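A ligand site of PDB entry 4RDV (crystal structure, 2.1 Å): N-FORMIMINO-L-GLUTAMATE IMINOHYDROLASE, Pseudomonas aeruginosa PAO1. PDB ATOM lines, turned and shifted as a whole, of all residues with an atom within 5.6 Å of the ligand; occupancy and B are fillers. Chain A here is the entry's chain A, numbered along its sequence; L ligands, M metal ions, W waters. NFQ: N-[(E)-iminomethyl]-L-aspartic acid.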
ATOM      1  N   HIS A  58      19.770  -5.349  -5.568  1.00  0.00           N
ATOM      2  CA  HIS A  58      18.520  -5.199  -6.350  1.00  0.00           C
ATOM      3  C   HIS A  58      18.861  -4.361  -7.580  1.00  0.00           C
ATOM      4  O   HIS A  58      18.867  -3.120  -7.516  1.00  0.00           O
ATOM      5  CB  HIS A  58      17.410  -4.504  -5.545  1.00  0.00           C
ATOM      6  CG  HIS A  58      17.246  -5.022  -4.152  1.00  0.00           C
ATOM      7  ND1 HIS A  58      16.902  -6.324  -3.874  1.00  0.00           N
ATOM      8  CD2 HIS A  58      17.376  -4.402  -2.960  1.00  0.00           C
ATOM      9  CE1 HIS A  58      16.821  -6.491  -2.558  1.00  0.00           C
ATOM     10  NE2 HIS A  58      17.100  -5.336  -1.989  1.00  0.00           N
ATOM     11  N   GLN A  61      17.587  -0.811  -9.031  1.00  0.00           N
ATOM     12  CA  GLN A  61      17.717   0.371  -8.188  1.00  0.00           C
ATOM     13  C   GLN A  61      18.901   1.282  -8.566  1.00  0.00           C
ATOM     14  O   GLN A  61      18.903   2.472  -8.228  1.00  0.00           O
ATOM     15  CB  GLN A  61      17.756  -0.027  -6.705  1.00  0.00           C
ATOM     16  CG  GLN A  61      16.446  -0.697  -6.263  1.00  0.00           C
ATOM     17  CD  GLN A  61      16.379  -0.956  -4.758  1.00  0.00           C
ATOM     18  OE1 GLN A  61      17.236  -0.518  -3.994  1.00  0.00           O
ATOM     19  NE2 GLN A  61      15.343  -1.679  -4.343  1.00  0.00           N
ATOM     20  N   PHE A  78      13.499   6.025   5.108  1.00  0.00           N
ATOM     21  CA  PHE A  78      13.398   4.755   4.399  1.00  0.00           C
ATOM     22  C   PHE A  78      12.028   4.574   3.762  1.00  0.00           C
ATOM     23  O   PHE A  78      11.909   4.103   2.639  1.00  0.00           O
ATOM     24  CB  PHE A  78      13.666   3.650   5.428  1.00  0.00           C
ATOM     25  CG  PHE A  78      13.450   2.251   4.919  1.00  0.00           C
ATOM     26  CD1 PHE A  78      14.536   1.457   4.586  1.00  0.00           C
ATOM     27  CD2 PHE A  78      12.174   1.710   4.832  1.00  0.00           C
ATOM     28  CE1 PHE A  78      14.346   0.154   4.139  1.00  0.00           C
ATOM     29  CE2 PHE A  78      11.968   0.413   4.384  1.00  0.00           C
ATOM     30  CZ  PHE A  78      13.060  -0.364   4.035  1.00  0.00           C
ATOM     31  N   TRP A  79      10.973   4.940   4.482  1.00  0.00           N
ATOM     32  CA  TRP A  79       9.607   4.689   4.019  1.00  0.00           C
ATOM     33  C   TRP A  79       9.150   5.644   2.922  1.00  0.00           C
ATOM     34  O   TRP A  79       8.439   5.231   2.012  1.00  0.00           O
ATOM     35  CB  TRP A  79       8.640   4.651   5.214  1.00  0.00           C
ATOM     36  CG  TRP A  79       9.084   3.617   6.212  1.00  0.00           C
ATOM     37  CD1 TRP A  79       9.818   3.836   7.348  1.00  0.00           C
ATOM     38  CD2 TRP A  79       8.891   2.199   6.131  1.00  0.00           C
ATOM     39  NE1 TRP A  79      10.059   2.647   7.991  1.00  0.00           N
ATOM     40  CE2 TRP A  79       9.511   1.625   7.266  1.00  0.00           C
ATOM     41  CE3 TRP A  79       8.243   1.358   5.210  1.00  0.00           C
ATOM     42  CZ2 TRP A  79       9.501   0.246   7.502  1.00  0.00           C
ATOM     43  CZ3 TRP A  79       8.233  -0.004   5.451  1.00  0.00           C
ATOM     44  CH2 TRP A  79       8.857  -0.549   6.588  1.00  0.00           C
ATOM     45  N   TRP A  81      11.353   6.979   0.907  1.00  0.00           N
ATOM     46  CA  TRP A  81      12.220   6.506  -0.166  1.00  0.00           C
ATOM     47  C   TRP A  81      11.586   5.316  -0.885  1.00  0.00           C
ATOM     48  O   TRP A  81      11.603   5.263  -2.119  1.00  0.00           O
ATOM     49  CB  TRP A  81      13.589   6.097   0.388  1.00  0.00           C
ATOM     50  CG  TRP A  81      14.428   5.327  -0.621  1.00  0.00           C
ATOM     51  CD1 TRP A  81      15.283   5.845  -1.544  1.00  0.00           C
ATOM     52  CD2 TRP A  81      14.483   3.899  -0.779  1.00  0.00           C
ATOM     53  NE1 TRP A  81      15.874   4.842  -2.267  1.00  0.00           N
ATOM     54  CE2 TRP A  81      15.387   3.632  -1.830  1.00  0.00           C
ATOM     55  CE3 TRP A  81      13.853   2.819  -0.149  1.00  0.00           C
ATOM     56  CZ2 TRP A  81      15.692   2.335  -2.253  1.00  0.00           C
ATOM     57  CZ3 TRP A  81      14.141   1.527  -0.572  1.00  0.00           C
ATOM     58  CH2 TRP A  81      15.052   1.299  -1.610  1.00  0.00           C
ATOM     59  N   ARG A  82      11.050   4.380  -0.118  1.00  0.00           N
ATOM     60  CA  ARG A  82      10.449   3.170  -0.706  1.00  0.00           C
ATOM     61  C   ARG A  82       9.286   3.517  -1.633  1.00  0.00           C
ATOM     62  O   ARG A  82       9.120   2.891  -2.668  1.00  0.00           O
ATOM     63  CB  ARG A  82      10.020   2.168   0.375  1.00  0.00           C
ATOM     64  CG  ARG A  82       9.823   0.734  -0.158  1.00  0.00           C
ATOM     65  CD  ARG A  82       9.374  -0.217   0.951  1.00  0.00           C
ATOM     66  NE  ARG A  82       7.996   0.038   1.397  1.00  0.00           N
ATOM     67  CZ  ARG A  82       7.259  -0.853   2.027  1.00  0.00           C
ATOM     68  NH1 ARG A  82       7.759  -2.054   2.297  1.00  0.00           N
ATOM     69  NH2 ARG A  82       6.008  -0.566   2.402  1.00  0.00           N
ATOM     70  N   MET A  85      10.885   4.440  -4.768  1.00  0.00           N
ATOM     71  CA  MET A  85      11.399   3.247  -5.432  1.00  0.00           C
ATOM     72  C   MET A  85      10.237   2.467  -6.076  1.00  0.00           C
ATOM     73  O   MET A  85      10.373   1.972  -7.191  1.00  0.00           O
ATOM     74  CB  MET A  85      12.237   2.386  -4.461  1.00  0.00           C
ATOM     75  CG  MET A  85      12.846   1.131  -5.087  1.00  0.00           C
ATOM     76  SD  MET A  85      11.756  -0.319  -5.033  1.00  0.00           S
ATOM     77  CE  MET A  85      11.748  -0.736  -3.294  1.00  0.00           C
ATOM     78  N   TYR A  86       9.079   2.412  -5.414  1.00  0.00           N
ATOM     79  CA  TYR A  86       7.890   1.758  -5.978  1.00  0.00           C
ATOM     80  C   TYR A  86       7.429   2.396  -7.306  1.00  0.00           C
ATOM     81  O   TYR A  86       7.065   1.709  -8.264  1.00  0.00           O
ATOM     82  CB  TYR A  86       6.720   1.776  -4.976  1.00  0.00           C
ATOM     83  CG  TYR A  86       6.786   0.726  -3.873  1.00  0.00           C
ATOM     84  CD1 TYR A  86       7.818  -0.208  -3.823  1.00  0.00           C
ATOM     85  CD2 TYR A  86       5.796   0.663  -2.896  1.00  0.00           C
ATOM     86  CE1 TYR A  86       7.870  -1.159  -2.811  1.00  0.00           C
ATOM     87  CE2 TYR A  86       5.833  -0.279  -1.897  1.00  0.00           C
ATOM     88  CZ  TYR A  86       6.858  -1.198  -1.859  1.00  0.00           C
ATOM     89  OH  TYR A  86       6.877  -2.138  -0.847  1.00  0.00           O
ATOM     90  N   TYR A 121      13.120  -9.586  -6.857  1.00  0.00           N
ATOM     91  CA  TYR A 121      11.670  -9.662  -6.564  1.00  0.00           C
ATOM     92  C   TYR A 121      10.743  -9.034  -7.616  1.00  0.00           C
ATOM     93  O   TYR A 121       9.544  -9.004  -7.424  1.00  0.00           O
ATOM     94  CB  TYR A 121      11.349  -9.068  -5.181  1.00  0.00           C
ATOM     95  CG  TYR A 121      11.876  -7.665  -4.968  1.00  0.00           C
ATOM     96  CD1 TYR A 121      11.321  -6.579  -5.628  1.00  0.00           C
ATOM     97  CD2 TYR A 121      12.938  -7.426  -4.098  1.00  0.00           C
ATOM     98  CE1 TYR A 121      11.805  -5.287  -5.431  1.00  0.00           C
ATOM     99  CE2 TYR A 121      13.437  -6.144  -3.887  1.00  0.00           C
ATOM    100  CZ  TYR A 121      12.858  -5.074  -4.555  1.00  0.00           C
ATOM    101  OH  TYR A 121      13.333  -3.808  -4.353  1.00  0.00           O
ATOM    102  N   TYR A 159       7.396 -13.065  -2.227  1.00  0.00           N
ATOM    103  CA  TYR A 159       6.846 -11.824  -1.709  1.00  0.00           C
ATOM    104  C   TYR A 159       5.330 -11.976  -1.856  1.00  0.00           C
ATOM    105  O   TYR A 159       4.838 -12.215  -2.955  1.00  0.00           O
ATOM    106  CB  TYR A 159       7.342 -10.664  -2.562  1.00  0.00           C
ATOM    107  CG  TYR A 159       7.226  -9.301  -1.933  1.00  0.00           C
ATOM    108  CD1 TYR A 159       8.349  -8.486  -1.774  1.00  0.00           C
ATOM    109  CD2 TYR A 159       5.984  -8.804  -1.493  1.00  0.00           C
ATOM    110  CE1 TYR A 159       8.260  -7.227  -1.195  1.00  0.00           C
ATOM    111  CE2 TYR A 159       5.887  -7.550  -0.917  1.00  0.00           C
ATOM    112  CZ  TYR A 159       7.024  -6.767  -0.773  1.00  0.00           C
ATOM    113  OH  TYR A 159       6.928  -5.513  -0.197  1.00  0.00           O
ATOM    114  N   HIS A 206      11.417 -12.273   1.064  1.00  0.00           N
ATOM    115  CA  HIS A 206      11.746 -10.855   1.042  1.00  0.00           C
ATOM    116  C   HIS A 206      12.033 -10.320   2.436  1.00  0.00           C
ATOM    117  O   HIS A 206      13.033  -9.648   2.656  1.00  0.00           O
ATOM    118  CB  HIS A 206      10.630 -10.025   0.400  1.00  0.00           C
ATOM    119  CG  HIS A 206      10.880  -8.547   0.491  1.00  0.00           C
ATOM    120  ND1 HIS A 206      10.476  -7.801   1.575  1.00  0.00           N
ATOM    121  CD2 HIS A 206      11.537  -7.687  -0.330  1.00  0.00           C
ATOM    122  CE1 HIS A 206      10.847  -6.537   1.408  1.00  0.00           C
ATOM    123  NE2 HIS A 206      11.489  -6.450   0.247  1.00  0.00           N
ATOM    124  N   SER A 207      11.140 -10.641   3.361  1.00  0.00           N
ATOM    125  CA  SER A 207      11.207 -10.164   4.741  1.00  0.00           C
ATOM    126  C   SER A 207      10.098 -10.866   5.518  1.00  0.00           C
ATOM    127  O   SER A 207       9.229 -11.512   4.927  1.00  0.00           O
ATOM    128  CB  SER A 207      10.961  -8.660   4.780  1.00  0.00           C
ATOM    129  OG  SER A 207       9.678  -8.356   4.227  1.00  0.00           O
ATOM    130  N   ARG A 209       7.864  -9.257   6.933  1.00  0.00           N
ATOM    131  CA  ARG A 209       6.705  -8.447   6.578  1.00  0.00           C
ATOM    132  C   ARG A 209       5.958  -9.034   5.380  1.00  0.00           C
ATOM    133  O   ARG A 209       4.728  -9.020   5.318  1.00  0.00           O
ATOM    134  CB  ARG A 209       7.110  -6.999   6.262  1.00  0.00           C
ATOM    135  CG  ARG A 209       7.458  -6.163   7.486  1.00  0.00           C
ATOM    136  CD  ARG A 209       8.235  -4.903   7.099  1.00  0.00           C
ATOM    137  NE  ARG A 209       9.608  -5.192   6.664  1.00  0.00           N
ATOM    138  CZ  ARG A 209      10.102  -4.894   5.467  1.00  0.00           C
ATOM    139  NH1 ARG A 209       9.329  -4.328   4.542  1.00  0.00           N
ATOM    140  NH2 ARG A 209      11.371  -5.176   5.178  1.00  0.00           N
ATOM    141  N   HIS A 232      15.670 -10.223   4.049  1.00  0.00           N
ATOM    142  CA  HIS A 232      15.886  -8.923   4.692  1.00  0.00           C
ATOM    143  C   HIS A 232      15.362  -9.063   6.103  1.00  0.00           C
ATOM    144  O   HIS A 232      14.246  -9.528   6.289  1.00  0.00           O
ATOM    145  CB  HIS A 232      15.024  -7.826   4.057  1.00  0.00           C
ATOM    146  CG  HIS A 232      15.462  -7.377   2.707  1.00  0.00           C
ATOM    147  ND1 HIS A 232      14.602  -7.351   1.622  1.00  0.00           N
ATOM    148  CD2 HIS A 232      16.633  -6.851   2.263  1.00  0.00           C
ATOM    149  CE1 HIS A 232      15.239  -6.856   0.569  1.00  0.00           C
ATOM    150  NE2 HIS A 232      16.472  -6.551   0.936  1.00  0.00           N
ATOM    151  N   GLU A 235      16.088  -4.346   9.382  1.00  0.00           N
ATOM    152  CA  GLU A 235      16.728  -3.160   8.799  1.00  0.00           C
ATOM    153  C   GLU A 235      16.264  -1.834   9.450  1.00  0.00           C
ATOM    154  O   GLU A 235      17.070  -0.941   9.713  1.00  0.00           O
ATOM    155  CB  GLU A 235      16.508  -3.120   7.283  1.00  0.00           C
ATOM    156  CG  GLU A 235      17.282  -1.996   6.586  1.00  0.00           C
ATOM    157  CD  GLU A 235      17.006  -1.886   5.091  1.00  0.00           C
ATOM    158  OE1 GLU A 235      16.125  -2.620   4.569  1.00  0.00           O
ATOM    159  OE2 GLU A 235      17.686  -1.076   4.422  1.00  0.00           O
ATOM    160  N   HIS A 269      21.089  -7.011   6.255  1.00  0.00           N
ATOM    161  CA  HIS A 269      21.045  -5.904   7.210  1.00  0.00           C
ATOM    162  C   HIS A 269      21.182  -6.341   8.670  1.00  0.00           C
ATOM    163  O   HIS A 269      22.207  -6.081   9.304  1.00  0.00           O
ATOM    164  CB  HIS A 269      19.825  -4.976   7.016  1.00  0.00           C
ATOM    165  CG  HIS A 269      19.612  -4.569   5.582  1.00  0.00           C
ATOM    166  ND1 HIS A 269      20.559  -3.910   4.847  1.00  0.00           N
ATOM    167  CD2 HIS A 269      18.553  -4.777   4.752  1.00  0.00           C
ATOM    168  CE1 HIS A 269      20.107  -3.711   3.618  1.00  0.00           C
ATOM    169  NE2 HIS A 269      18.892  -4.233   3.537  1.00  0.00           N
ATOM    170  N   THR A 294      24.239   1.691   1.617  1.00  0.00           N
ATOM    171  CA  THR A 294      22.785   1.798   1.497  1.00  0.00           C
ATOM    172  C   THR A 294      22.150   2.053   2.866  1.00  0.00           C
ATOM    173  O   THR A 294      21.243   2.881   3.007  1.00  0.00           O
ATOM    174  CB  THR A 294      22.167   0.550   0.813  1.00  0.00           C
ATOM    175  OG1 THR A 294      22.524   0.537  -0.575  1.00  0.00           O
ATOM    176  CG2 THR A 294      20.626   0.558   0.935  1.00  0.00           C
ATOM    177  N   LEU A 298      19.929   5.209   3.606  1.00  0.00           N
ATOM    178  CA  LEU A 298      18.516   5.051   3.997  1.00  0.00           C
ATOM    179  C   LEU A 298      18.248   5.386   5.465  1.00  0.00           C
ATOM    180  O   LEU A 298      17.105   5.276   5.933  1.00  0.00           O
ATOM    181  CB  LEU A 298      18.033   3.628   3.694  1.00  0.00           C
ATOM    182  CG  LEU A 298      18.041   3.276   2.205  1.00  0.00           C
ATOM    183  CD1 LEU A 298      17.563   1.835   1.964  1.00  0.00           C
ATOM    184  CD2 LEU A 298      17.158   4.267   1.439  1.00  0.00           C
ATOM    185  N   ASP A 300      19.248   3.652   8.132  1.00  0.00           N
ATOM    186  CA  ASP A 300      18.886   2.450   8.862  1.00  0.00           C
ATOM    187  C   ASP A 300      19.490   2.405  10.260  1.00  0.00           C
ATOM    188  O   ASP A 300      18.831   2.021  11.224  1.00  0.00           O
ATOM    189  CB  ASP A 300      19.333   1.213   8.073  1.00  0.00           C
ATOM    190  CG  ASP A 300      18.555   1.016   6.796  1.00  0.00           C
ATOM    191  OD1 ASP A 300      17.374   1.415   6.723  1.00  0.00           O
ATOM    192  OD2 ASP A 300      19.135   0.439   5.851  1.00  0.00           O
ATOM    193  N   ASP A 320      23.443  -3.465  -2.502  1.00  0.00           N
ATOM    194  CA  ASP A 320      22.012  -3.286  -2.234  1.00  0.00           C
ATOM    195  C   ASP A 320      21.274  -2.342  -3.189  1.00  0.00           C
ATOM    196  O   ASP A 320      20.873  -2.748  -4.283  1.00  0.00           O
ATOM    197  CB  ASP A 320      21.788  -2.851  -0.768  1.00  0.00           C
ATOM    198  CG  ASP A 320      20.339  -2.936  -0.344  1.00  0.00           C
ATOM    199  OD1 ASP A 320      19.498  -3.418  -1.141  1.00  0.00           O
ATOM    200  OD2 ASP A 320      20.015  -2.548   0.798  1.00  0.00           O
HETATM  201  C   NFQ L   1      13.541  -3.612  -0.944  1.00  0.00           C
HETATM  202  N   NFQ L   1      14.960  -2.213   0.328  1.00  0.00           N
HETATM  203  O1  NFQ L   1      14.209  -3.163  -1.917  1.00  0.00           O
HETATM  204  O2  NFQ L   1      12.621  -4.443  -1.143  1.00  0.00           O
HETATM  205  CA  NFQ L   1      13.875  -3.135   0.431  1.00  0.00           C
HETATM  206  CB  NFQ L   1      12.660  -2.476   1.019  1.00  0.00           C
HETATM  207  CF  NFQ L   1      15.593  -1.941   1.580  1.00  0.00           C
HETATM  208  NF  NFQ L   1      16.698  -1.225   1.543  1.00  0.00           N
HETATM  209  CG  NFQ L   1      11.816  -3.324   1.918  1.00  0.00           C
HETATM  210  OD1 NFQ L   1      10.554  -3.279   1.846  1.00  0.00           O
HETATM  211  OD2 NFQ L   1      12.380  -4.103   2.739  1.00  0.00           O
HETATM  212 ZN    ZN M   1      17.795  -5.299  -0.124  1.00  0.00          ZN
HETATM  213  O   HOH W   1      17.888  -3.874   1.196  1.00  0.00           O
HETATM  214  O   HOH W   2       9.018  -3.972  -0.371  1.00  0.00           O
HETATM  215  O   HOH W   3      10.476  -4.214  -2.485  1.00  0.00           O
HETATM  216  O   HOH W   4      17.327  -1.366  -1.302  1.00  0.00           O
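The side-chain hydroxyl (OH) of Tyr 121 sits at hydrogen-bond distance from an oxygen (O1) of the ligand (2.7 Å). An oxygen (O2) of the ligand is in hydrogen-bond range of a ring nitrogen (NE2) of His 206 (2.7 Å). The guanidinium group (NH2) of Arg 209 is in salt-bridge range of an oxygen (OD2) of the ligand, at 2.8 Å. OE2 of Glu 235 is in salt-bridge range of NF of the ligand, 3.0 Å away. An oxygen (O1) of the ligand sits at hydrogen-bond distance from the side-chain amide nitrogen (NE2) of Gln 61 (3.1 Å). OD1 of the ligand is in salt-bridge range of NH1 of Arg 82 (3.1 Å). NF of the ligand lies within salt-bridge range of OD2 of Asp 320 (3.6 Å).
The side-chain hydroxyl (OH) of Tyr 121 sits at hydrogen-bond distance from the side-chain amide nitrogen (NE2) of Gln 61 (2.9 Å). The backbone carbonyl oxygen (O) of His 206 sits at hydrogen-bond distance from a ring nitrogen (ND1) of His 232 (3.0 Å). The side-chain hydroxyl (OG) of Ser 207 is in hydrogen-bond range of a ring nitrogen (ND1) of His 206 (2.8 Å). N of Arg 209 sits close to OG of Ser 207, at 3.4 Å. The side-chain carboxylate of Glu 235 lies close to the side-chain carboxylate of Asp 300, at 2.5 Å. NH1 of Arg 82 sits close to OH of Tyr 86, 3.3 Å away. N of His 58 is in hydrogen-bond range of O of Asp 320 (3.1 Å). The side-chain carboxylate (OD2) of Asp 320 sits close to a ring nitrogen (NE2) of His 269 (3.4 Å).
His 58 touches the ligand (CD2 to O1, 3.6 Å). Phe 78 touches the ligand. CZ3 of Trp 81 touches N of the ligand, 3.9 Å away. CE of Met 85 touches O1 of the ligand, 3.7 Å away. CE1 of His 232 touches O2 of the ligand, 3.95 Å away. CD1 of Leu 298 touches NF of the ligand, 3.2 Å away. Hydrophobic or aromatic side chains that line the ligand: His 58, Phe 78, Trp 81, Met 85, Tyr 121, His 206, His 232 and Leu 298. Along chain A the residues within 4 Å of the ligand span positions 58 to 320. The nearest printed residue that does not touch the ligand is His 269 (4.2 Å).
Water W3 lies within hydrogen-bond range of an oxygen (O2) of the ligand and the side-chain hydroxyl (OH) of Tyr 121. Water W2 lies within hydrogen-bond range of OH of Tyr 159, OD1 of the ligand and OH of Tyr 86. Water W4 lies within hydrogen-bond range of the side-chain amide oxygen (OE1) of Gln 61 (2.8 Å), a nitrogen (NF) of the ligand (2.9 Å) and the side-chain carboxylate (OD1) of Asp 320 (3.0 Å). Water W1 lies within hydrogen-bond range of OD2 of Asp 320, NE2 of His 269 and NF of the ligand.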
